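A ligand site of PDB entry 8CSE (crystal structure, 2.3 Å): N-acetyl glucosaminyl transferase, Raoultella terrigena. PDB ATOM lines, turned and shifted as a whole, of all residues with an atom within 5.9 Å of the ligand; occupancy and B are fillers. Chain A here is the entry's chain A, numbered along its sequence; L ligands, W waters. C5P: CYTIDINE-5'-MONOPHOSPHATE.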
ATOM      1  N   PRO A 162      20.760   0.480  11.412  1.00  0.00           N
ATOM      2  CA  PRO A 162      20.894  -0.862  10.857  1.00  0.00           C
ATOM      3  C   PRO A 162      20.896  -0.892   9.333  1.00  0.00           C
ATOM      4  O   PRO A 162      21.275  -1.923   8.770  1.00  0.00           O
ATOM      5  CB  PRO A 162      19.653  -1.577  11.404  1.00  0.00           C
ATOM      6  CG  PRO A 162      18.630  -0.476  11.471  1.00  0.00           C
ATOM      7  CD  PRO A 162      19.368   0.800  11.775  1.00  0.00           C
ATOM      8  N   LEU A 163      20.467   0.166   8.676  1.00  0.00           N
ATOM      9  CA  LEU A 163      20.530   0.289   7.224  1.00  0.00           C
ATOM     10  C   LEU A 163      21.597   1.321   6.887  1.00  0.00           C
ATOM     11  O   LEU A 163      21.569   2.444   7.419  1.00  0.00           O
ATOM     12  CB  LEU A 163      19.165   0.686   6.637  1.00  0.00           C
ATOM     13  CG  LEU A 163      18.079  -0.353   6.920  1.00  0.00           C
ATOM     14  CD1 LEU A 163      16.674   0.147   6.556  1.00  0.00           C
ATOM     15  CD2 LEU A 163      18.374  -1.686   6.207  1.00  0.00           C
ATOM     16  N   ARG A 164      22.537   0.942   6.010  1.00  0.00           N
ATOM     17  CA  ARG A 164      23.785   1.659   5.794  1.00  0.00           C
ATOM     18  C   ARG A 164      24.189   1.563   4.326  1.00  0.00           C
ATOM     19  O   ARG A 164      23.892   0.597   3.637  1.00  0.00           O
ATOM     20  CB  ARG A 164      24.930   1.064   6.611  1.00  0.00           C
ATOM     21  CG  ARG A 164      24.661   0.962   8.079  1.00  0.00           C
ATOM     22  CD  ARG A 164      25.688   0.089   8.780  1.00  0.00           C
ATOM     23  NE  ARG A 164      25.262  -0.105  10.151  1.00  0.00           N
ATOM     24  CZ  ARG A 164      26.002  -0.688  11.077  1.00  0.00           C
ATOM     25  NH1 ARG A 164      27.205  -1.169  10.781  1.00  0.00           N
ATOM     26  NH2 ARG A 164      25.541  -0.770  12.331  1.00  0.00           N
ATOM     27  N   MET A 167      24.522  -0.403   0.351  1.00  0.00           N
ATOM     28  CA  MET A 167      23.290  -1.113   0.006  1.00  0.00           C
ATOM     29  C   MET A 167      22.065  -0.223   0.199  1.00  0.00           C
ATOM     30  O   MET A 167      21.074  -0.336  -0.544  1.00  0.00           O
ATOM     31  CB  MET A 167      23.139  -2.388   0.849  1.00  0.00           C
ATOM     32  CG  MET A 167      24.247  -3.445   0.693  1.00  0.00           C
ATOM     33  SD  MET A 167      24.173  -4.207  -0.905  1.00  0.00           S
ATOM     34  CE  MET A 167      22.700  -5.168  -0.966  1.00  0.00           C
ATOM     35  N   TYR A 168      22.106   0.655   1.204  1.00  0.00           N
ATOM     36  CA  TYR A 168      20.942   1.387   1.682  1.00  0.00           C
ATOM     37  C   TYR A 168      21.281   2.869   1.863  1.00  0.00           C
ATOM     38  O   TYR A 168      22.443   3.251   1.990  1.00  0.00           O
ATOM     39  CB  TYR A 168      20.451   0.798   3.018  1.00  0.00           C
ATOM     40  CG  TYR A 168      20.098  -0.663   2.928  1.00  0.00           C
ATOM     41  CD1 TYR A 168      18.891  -1.060   2.362  1.00  0.00           C
ATOM     42  CD2 TYR A 168      20.959  -1.655   3.396  1.00  0.00           C
ATOM     43  CE1 TYR A 168      18.535  -2.386   2.270  1.00  0.00           C
ATOM     44  CE2 TYR A 168      20.599  -3.012   3.308  1.00  0.00           C
ATOM     45  CZ  TYR A 168      19.380  -3.360   2.738  1.00  0.00           C
ATOM     46  OH  TYR A 168      18.975  -4.669   2.619  1.00  0.00           O
ATOM     47  N   VAL A 226      22.648 -18.519   9.634  1.00  0.00           N
ATOM     48  CA  VAL A 226      23.154 -18.056  10.922  1.00  0.00           C
ATOM     49  C   VAL A 226      23.980 -16.795  10.696  1.00  0.00           C
ATOM     50  O   VAL A 226      25.022 -16.828  10.005  1.00  0.00           O
ATOM     51  CB  VAL A 226      23.983 -19.142  11.616  1.00  0.00           C
ATOM     52  CG1 VAL A 226      24.348 -18.706  13.054  1.00  0.00           C
ATOM     53  CG2 VAL A 226      23.215 -20.450  11.620  1.00  0.00           C
ATOM     54  N   VAL A 227      23.524 -15.675  11.250  1.00  0.00           N
ATOM     55  CA  VAL A 227      24.237 -14.405  11.215  1.00  0.00           C
ATOM     56  C   VAL A 227      25.170 -14.343  12.413  1.00  0.00           C
ATOM     57  O   VAL A 227      24.725 -14.379  13.554  1.00  0.00           O
ATOM     58  CB  VAL A 227      23.277 -13.220  11.242  1.00  0.00           C
ATOM     59  CG1 VAL A 227      24.082 -11.878  11.185  1.00  0.00           C
ATOM     60  CG2 VAL A 227      22.229 -13.314  10.116  1.00  0.00           C
ATOM     61  N   LEU A 228      26.480 -14.231  12.162  1.00  0.00           N
ATOM     62  CA  LEU A 228      27.428 -13.979  13.234  1.00  0.00           C
ATOM     63  C   LEU A 228      27.699 -12.488  13.333  1.00  0.00           C
ATOM     64  O   LEU A 228      27.515 -11.727  12.375  1.00  0.00           O
ATOM     65  CB  LEU A 228      28.724 -14.756  12.990  1.00  0.00           C
ATOM     66  CG  LEU A 228      28.507 -16.271  12.762  1.00  0.00           C
ATOM     67  CD1 LEU A 228      29.815 -17.052  12.695  1.00  0.00           C
ATOM     68  CD2 LEU A 228      27.564 -16.841  13.809  1.00  0.00           C
ATOM     69  N   GLN A 229      28.176 -12.068  14.512  1.00  0.00           N
ATOM     70  CA  GLN A 229      28.427 -10.671  14.788  1.00  0.00           C
ATOM     71  C   GLN A 229      29.858 -10.463  15.205  1.00  0.00           C
ATOM     72  O   GLN A 229      30.613 -11.425  15.365  1.00  0.00           O
ATOM     73  CB  GLN A 229      27.457 -10.175  15.857  1.00  0.00           C
ATOM     74  CG  GLN A 229      26.096  -9.840  15.225  1.00  0.00           C
ATOM     75  CD  GLN A 229      25.017  -9.581  16.256  1.00  0.00           C
ATOM     76  OE1 GLN A 229      24.283 -10.504  16.641  1.00  0.00           O
ATOM     77  NE2 GLN A 229      24.871  -8.312  16.658  1.00  0.00           N
ATOM     78  N   VAL A 230      30.241  -9.200  15.400  1.00  0.00           N
ATOM     79  CA  VAL A 230      31.556  -8.910  15.971  1.00  0.00           C
ATOM     80  C   VAL A 230      31.548  -9.254  17.465  1.00  0.00           C
ATOM     81  O   VAL A 230      30.596  -8.923  18.197  1.00  0.00           O
ATOM     82  CB  VAL A 230      31.955  -7.447  15.710  1.00  0.00           C
ATOM     83  CG1 VAL A 230      33.301  -7.133  16.395  1.00  0.00           C
ATOM     84  CG2 VAL A 230      32.074  -7.151  14.201  1.00  0.00           C
ATOM     85  N   ASP A 233      31.426  -6.357  19.984  1.00  0.00           N
ATOM     86  CA  ASP A 233      30.370  -5.365  19.769  1.00  0.00           C
ATOM     87  C   ASP A 233      29.576  -5.137  21.063  1.00  0.00           C
ATOM     88  O   ASP A 233      29.276  -6.096  21.765  1.00  0.00           O
ATOM     89  CB  ASP A 233      29.463  -5.916  18.644  1.00  0.00           C
ATOM     90  CG  ASP A 233      28.382  -4.946  18.149  1.00  0.00           C
ATOM     91  OD1 ASP A 233      27.772  -4.207  18.950  1.00  0.00           O
ATOM     92  OD2 ASP A 233      28.095  -4.969  16.930  1.00  0.00           O
ATOM     93  N   ASN A 235      26.620  -4.769  21.364  1.00  0.00           N
ATOM     94  CA  ASN A 235      25.467  -5.628  21.164  1.00  0.00           C
ATOM     95  C   ASN A 235      25.673  -7.049  21.690  1.00  0.00           C
ATOM     96  O   ASN A 235      24.737  -7.675  22.184  1.00  0.00           O
ATOM     97  CB  ASN A 235      25.107  -5.679  19.676  1.00  0.00           C
ATOM     98  CG  ASN A 235      24.147  -4.567  19.251  1.00  0.00           C
ATOM     99  OD1 ASN A 235      23.515  -3.941  20.072  1.00  0.00           O
ATOM    100  ND2 ASN A 235      24.057  -4.333  17.965  1.00  0.00           N
ATOM    101  N   ARG A 264      27.294 -17.123   8.053  1.00  0.00           N
ATOM    102  CA  ARG A 264      27.977 -15.943   7.519  1.00  0.00           C
ATOM    103  C   ARG A 264      28.636 -15.187   8.665  1.00  0.00           C
ATOM    104  O   ARG A 264      27.954 -14.612   9.526  1.00  0.00           O
ATOM    105  CB  ARG A 264      27.013 -15.017   6.773  1.00  0.00           C
ATOM    106  CG  ARG A 264      27.625 -13.676   6.470  1.00  0.00           C
ATOM    107  CD  ARG A 264      26.766 -12.948   5.492  1.00  0.00           C
ATOM    108  NE  ARG A 264      27.299 -11.617   5.242  1.00  0.00           N
ATOM    109  CZ  ARG A 264      28.053 -11.307   4.199  1.00  0.00           C
ATOM    110  NH1 ARG A 264      28.359 -12.212   3.272  1.00  0.00           N
ATOM    111  NH2 ARG A 264      28.507 -10.046   4.091  1.00  0.00           N
ATOM    112  N   ALA A 265      29.966 -15.177   8.657  1.00  0.00           N
ATOM    113  CA  ALA A 265      30.757 -14.418   9.608  1.00  0.00           C
ATOM    114  C   ALA A 265      30.577 -12.924   9.355  1.00  0.00           C
ATOM    115  O   ALA A 265      30.214 -12.501   8.250  1.00  0.00           O
ATOM    116  CB  ALA A 265      32.227 -14.832   9.482  1.00  0.00           C
ATOM    117  N   HIS A 266      30.779 -12.119  10.375  1.00  0.00           N
ATOM    118  CA  HIS A 266      30.684 -10.663  10.205  1.00  0.00           C
ATOM    119  C   HIS A 266      31.956 -10.173   9.530  1.00  0.00           C
ATOM    120  O   HIS A 266      33.048 -10.537   9.975  1.00  0.00           O
ATOM    121  CB  HIS A 266      30.524  -9.960  11.558  1.00  0.00           C
ATOM    122  CG  HIS A 266      30.164  -8.497  11.468  1.00  0.00           C
ATOM    123  ND1 HIS A 266      31.024  -7.542  10.959  1.00  0.00           N
ATOM    124  CD2 HIS A 266      29.051  -7.818  11.866  1.00  0.00           C
ATOM    125  CE1 HIS A 266      30.448  -6.344  11.032  1.00  0.00           C
ATOM    126  NE2 HIS A 266      29.253  -6.489  11.574  1.00  0.00           N
ATOM    127  N   PRO A 267      31.873  -9.354   8.488  1.00  0.00           N
ATOM    128  CA  PRO A 267      33.103  -8.908   7.834  1.00  0.00           C
ATOM    129  C   PRO A 267      33.965  -7.986   8.680  1.00  0.00           C
ATOM    130  O   PRO A 267      35.165  -7.869   8.395  1.00  0.00           O
ATOM    131  CB  PRO A 267      32.578  -8.209   6.565  1.00  0.00           C
ATOM    132  CG  PRO A 267      31.175  -8.744   6.365  1.00  0.00           C
ATOM    133  CD  PRO A 267      30.672  -8.897   7.780  1.00  0.00           C
ATOM    134  N   ASN A 285      27.325  -9.430   0.045  1.00  0.00           N
ATOM    135  CA  ASN A 285      26.641  -8.586   1.018  1.00  0.00           C
ATOM    136  C   ASN A 285      25.641  -9.429   1.811  1.00  0.00           C
ATOM    137  O   ASN A 285      25.233 -10.501   1.355  1.00  0.00           O
ATOM    138  CB  ASN A 285      25.942  -7.404   0.328  1.00  0.00           C
ATOM    139  CG  ASN A 285      25.009  -7.845  -0.761  1.00  0.00           C
ATOM    140  OD1 ASN A 285      23.962  -8.441  -0.487  1.00  0.00           O
ATOM    141  ND2 ASN A 285      25.385  -7.597  -2.007  1.00  0.00           N
ATOM    142  N   SER A 286      25.222  -8.929   2.988  1.00  0.00           N
ATOM    143  CA  SER A 286      24.296  -9.749   3.780  1.00  0.00           C
ATOM    144  C   SER A 286      22.972  -9.977   3.092  1.00  0.00           C
ATOM    145  O   SER A 286      22.282 -10.959   3.419  1.00  0.00           O
ATOM    146  CB  SER A 286      24.034  -9.139   5.165  1.00  0.00           C
ATOM    147  OG  SER A 286      23.663  -7.773   5.108  1.00  0.00           O
ATOM    148  N   ASN A 300      21.389 -10.137  17.676  1.00  0.00           N
ATOM    149  CA  ASN A 300      20.779  -8.817  17.473  1.00  0.00           C
ATOM    150  C   ASN A 300      21.490  -8.011  16.393  1.00  0.00           C
ATOM    151  O   ASN A 300      21.617  -6.783  16.498  1.00  0.00           O
ATOM    152  CB  ASN A 300      20.725  -8.041  18.799  1.00  0.00           C
ATOM    153  CG  ASN A 300      22.028  -8.068  19.565  1.00  0.00           C
ATOM    154  OD1 ASN A 300      23.119  -8.245  18.979  1.00  0.00           O
ATOM    155  ND2 ASN A 300      21.934  -7.874  20.890  1.00  0.00           N
ATOM    156  N   SER A 301      21.927  -8.688  15.334  1.00  0.00           N
ATOM    157  CA  SER A 301      22.523  -8.035  14.177  1.00  0.00           C
ATOM    158  C   SER A 301      21.549  -7.130  13.440  1.00  0.00           C
ATOM    159  O   SER A 301      20.348  -7.409  13.333  1.00  0.00           O
ATOM    160  CB  SER A 301      23.017  -9.085  13.176  1.00  0.00           C
ATOM    161  OG  SER A 301      23.537  -8.463  12.030  1.00  0.00           O
ATOM    162  N   SER A 302      22.103  -6.052  12.880  1.00  0.00           N
ATOM    163  CA  SER A 302      21.373  -5.290  11.872  1.00  0.00           C
ATOM    164  C   SER A 302      20.765  -6.176  10.796  1.00  0.00           C
ATOM    165  O   SER A 302      19.685  -5.850  10.274  1.00  0.00           O
ATOM    166  CB  SER A 302      22.303  -4.261  11.239  1.00  0.00           C
ATOM    167  OG  SER A 302      22.832  -3.381  12.219  1.00  0.00           O
ATOM    168  N   VAL A 303      21.405  -7.293  10.459  1.00  0.00           N
ATOM    169  CA  VAL A 303      20.895  -8.167   9.408  1.00  0.00           C
ATOM    170  C   VAL A 303      19.535  -8.743   9.758  1.00  0.00           C
ATOM    171  O   VAL A 303      18.721  -9.000   8.868  1.00  0.00           O
ATOM    172  CB  VAL A 303      21.934  -9.271   9.112  1.00  0.00           C
ATOM    173  CG1 VAL A 303      21.399 -10.256   8.011  1.00  0.00           C
ATOM    174  CG2 VAL A 303      23.292  -8.636   8.705  1.00  0.00           C
ATOM    175  N   GLU A 306      17.031  -6.782   8.091  1.00  0.00           N
ATOM    176  CA  GLU A 306      16.997  -7.077   6.661  1.00  0.00           C
ATOM    177  C   GLU A 306      16.164  -8.318   6.394  1.00  0.00           C
ATOM    178  O   GLU A 306      15.302  -8.331   5.506  1.00  0.00           O
ATOM    179  CB  GLU A 306      18.402  -7.288   6.105  1.00  0.00           C
ATOM    180  CG  GLU A 306      19.104  -6.085   5.565  1.00  0.00           C
ATOM    181  CD  GLU A 306      20.425  -6.472   4.904  1.00  0.00           C
ATOM    182  OE1 GLU A 306      21.254  -7.101   5.589  1.00  0.00           O
ATOM    183  OE2 GLU A 306      20.614  -6.177   3.715  1.00  0.00           O
HETATM  184  O3P C5P L   1      25.509  -7.217  12.806  1.00  0.00           O
HETATM  185  P   C5P L   1      25.769  -5.737  12.789  1.00  0.00           P
HETATM  186  O1P C5P L   1      24.615  -4.869  13.260  1.00  0.00           O
HETATM  187  O2P C5P L   1      27.139  -5.253  13.219  1.00  0.00           O
HETATM  188  O5' C5P L   1      25.725  -5.408  11.022  1.00  0.00           O
HETATM  189  C5' C5P L   1      26.110  -4.257  10.489  1.00  0.00           C
HETATM  190  C4' C5P L   1      26.414  -4.444   8.974  1.00  0.00           C
HETATM  191  O4' C5P L   1      27.326  -5.486   8.717  1.00  0.00           O
HETATM  192  C3' C5P L   1      25.081  -4.922   8.336  1.00  0.00           C
HETATM  193  O3' C5P L   1      24.180  -4.032   7.820  1.00  0.00           O
HETATM  194  C2' C5P L   1      25.578  -5.781   7.135  1.00  0.00           C
HETATM  195  O2' C5P L   1      25.881  -4.937   6.102  1.00  0.00           O
HETATM  196  C1' C5P L   1      26.957  -6.315   7.628  1.00  0.00           C
HETATM  197  N1  C5P L   1      26.987  -7.707   8.174  1.00  0.00           N
HETATM  198  C2  C5P L   1      27.321  -8.736   7.236  1.00  0.00           C
HETATM  199  N3  C5P L   1      27.366 -10.065   7.733  1.00  0.00           N
HETATM  200  C4  C5P L   1      27.125 -10.346   9.053  1.00  0.00           C
HETATM  201  C5  C5P L   1      26.766  -9.251   9.978  1.00  0.00           C
HETATM  202  C6  C5P L   1      26.742  -7.969   9.488  1.00  0.00           C
HETATM  203  O2  C5P L   1      27.521  -8.415   6.104  1.00  0.00           O
HETATM  204  N4  C5P L   1      27.166 -11.722   9.489  1.00  0.00           N
HETATM  205  O   HOH W   1      21.851  -5.444   7.527  1.00  0.00           O
HETATM  206  O   HOH W   2      25.412  -5.674  16.157  1.00  0.00           O
HETATM  207  O   HOH W   3      26.504  -6.706   3.826  1.00  0.00           O
HETATM  208  O   HOH W   4      24.120  -3.729   4.394  1.00  0.00           O
HETATM  209  O   HOH W   5      22.901  -1.924   6.090  1.00  0.00           O
HETATM  210  O   HOH W   6      28.503  -6.655  15.121  1.00  0.00           O
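OG of Ser 301 sits at hydrogen-bond distance from O3P of the ligand.
The backbone NH (N) of Ser 302 sits at hydrogen-bond distance from an oxygen (O1P) of the ligand, 2.8 Å away.
The side-chain hydroxyl (OG) of Ser 302 sits at hydrogen-bond distance from an oxygen (O1P) of the ligand, 2.5 Å away.
O of Arg 264 is in hydrogen-bond range of N4 of the ligand (3.0 Å).
NH2 of Arg 264 lies within hydrogen-bond range of O2 of the ligand (2.8 Å).
N4 of the ligand is in hydrogen-bond range of O of Leu 228.
A ring nitrogen (NE2) of His 266 lies within hydrogen-bond range of an oxygen (O2P) of the ligand (3.0 Å).
O of Ala 265 lies within hydrogen-bond range of N4 of the ligand (3.4 Å).
OG of Ser 301 lies within hydrogen-bond range of N of Val 303.
The backbone NH of Ser 301 lies within hydrogen-bond range of the side-chain amide oxygen of Gln 229.
O of Arg 264 lies within hydrogen-bond range of N of Leu 228, 3.0 Å away.
N of Arg 264 is in hydrogen-bond range of O of Val 226 (3.0 Å).
The side-chain hydroxyl of Ser 286 is in hydrogen-bond range of the side-chain carboxylate of Glu 306, 2.5 Å away.
The side-chain amide nitrogen (NE2) of Gln 229 sits at hydrogen-bond distance from the side-chain amide oxygen (OD1) of Asn 300.
OD1 of Asp 233 is in hydrogen-bond range of N of Asn 235 (2.7 Å).
Pro 162 touches the ligand.
Arg 164 touches the ligand (NH1 to C5', 3.3 Å).
Val 227 touches the ligand (CG1 to N4, 3.5 Å).
Gln 229 touches the ligand.
Asp 233 touches the ligand.
CD of Pro 267 touches C2 of the ligand, 3.4 Å away.
OG of Ser 286 touches C2' of the ligand (3.4 Å).
Val 303 touches the ligand (CG2 to C6, 3.6 Å).
Hydrophobic or aromatic side chains within 4 Å of the ligand: Val 227, His 266, Pro 267 and Val 303.
14 residues have an atom within 4 Å of the ligand: Pro 162, Arg 164, Val 227, Leu 228, Gln 229, Asp 233, Arg 264, Ala 265, His 266, Pro 267, Ser 286, Ser 301, Ser 302 and Val 303.
The nearest printed residue that does not touch the ligand is Asn 235 (4.8 Å).
Water W6 lies within hydrogen-bond range of the side-chain carboxylate of Asp 233 (2.5 Å), an oxygen (O2P) of the ligand (2.7 Å) and the backbone NH of Val 230 (3.1 Å).
Water W1 lies within hydrogen-bond range of OE1 of Glu 306, O3' of the ligand and N of Val 303.
Water W3 bridges the backbone NH (N) of Ser 286 (2.7 Å) and an oxygen (O2') of the ligand (2.9 Å).
Water W5 lies within hydrogen-bond range of the backbone NH (N) of Arg 164 (2.9 Å), an oxygen (O3') of the ligand (3.0 Å) and the backbone carbonyl oxygen (O) of Pro 162 (3.1 Å).
Water W2 lies within hydrogen-bond range of the side-chain amide nitrogen of Asn 235, the side-chain amide nitrogen of Gln 229, the side-chain carboxylate of Asp 233 and an oxygen (O1P) of the ligand.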
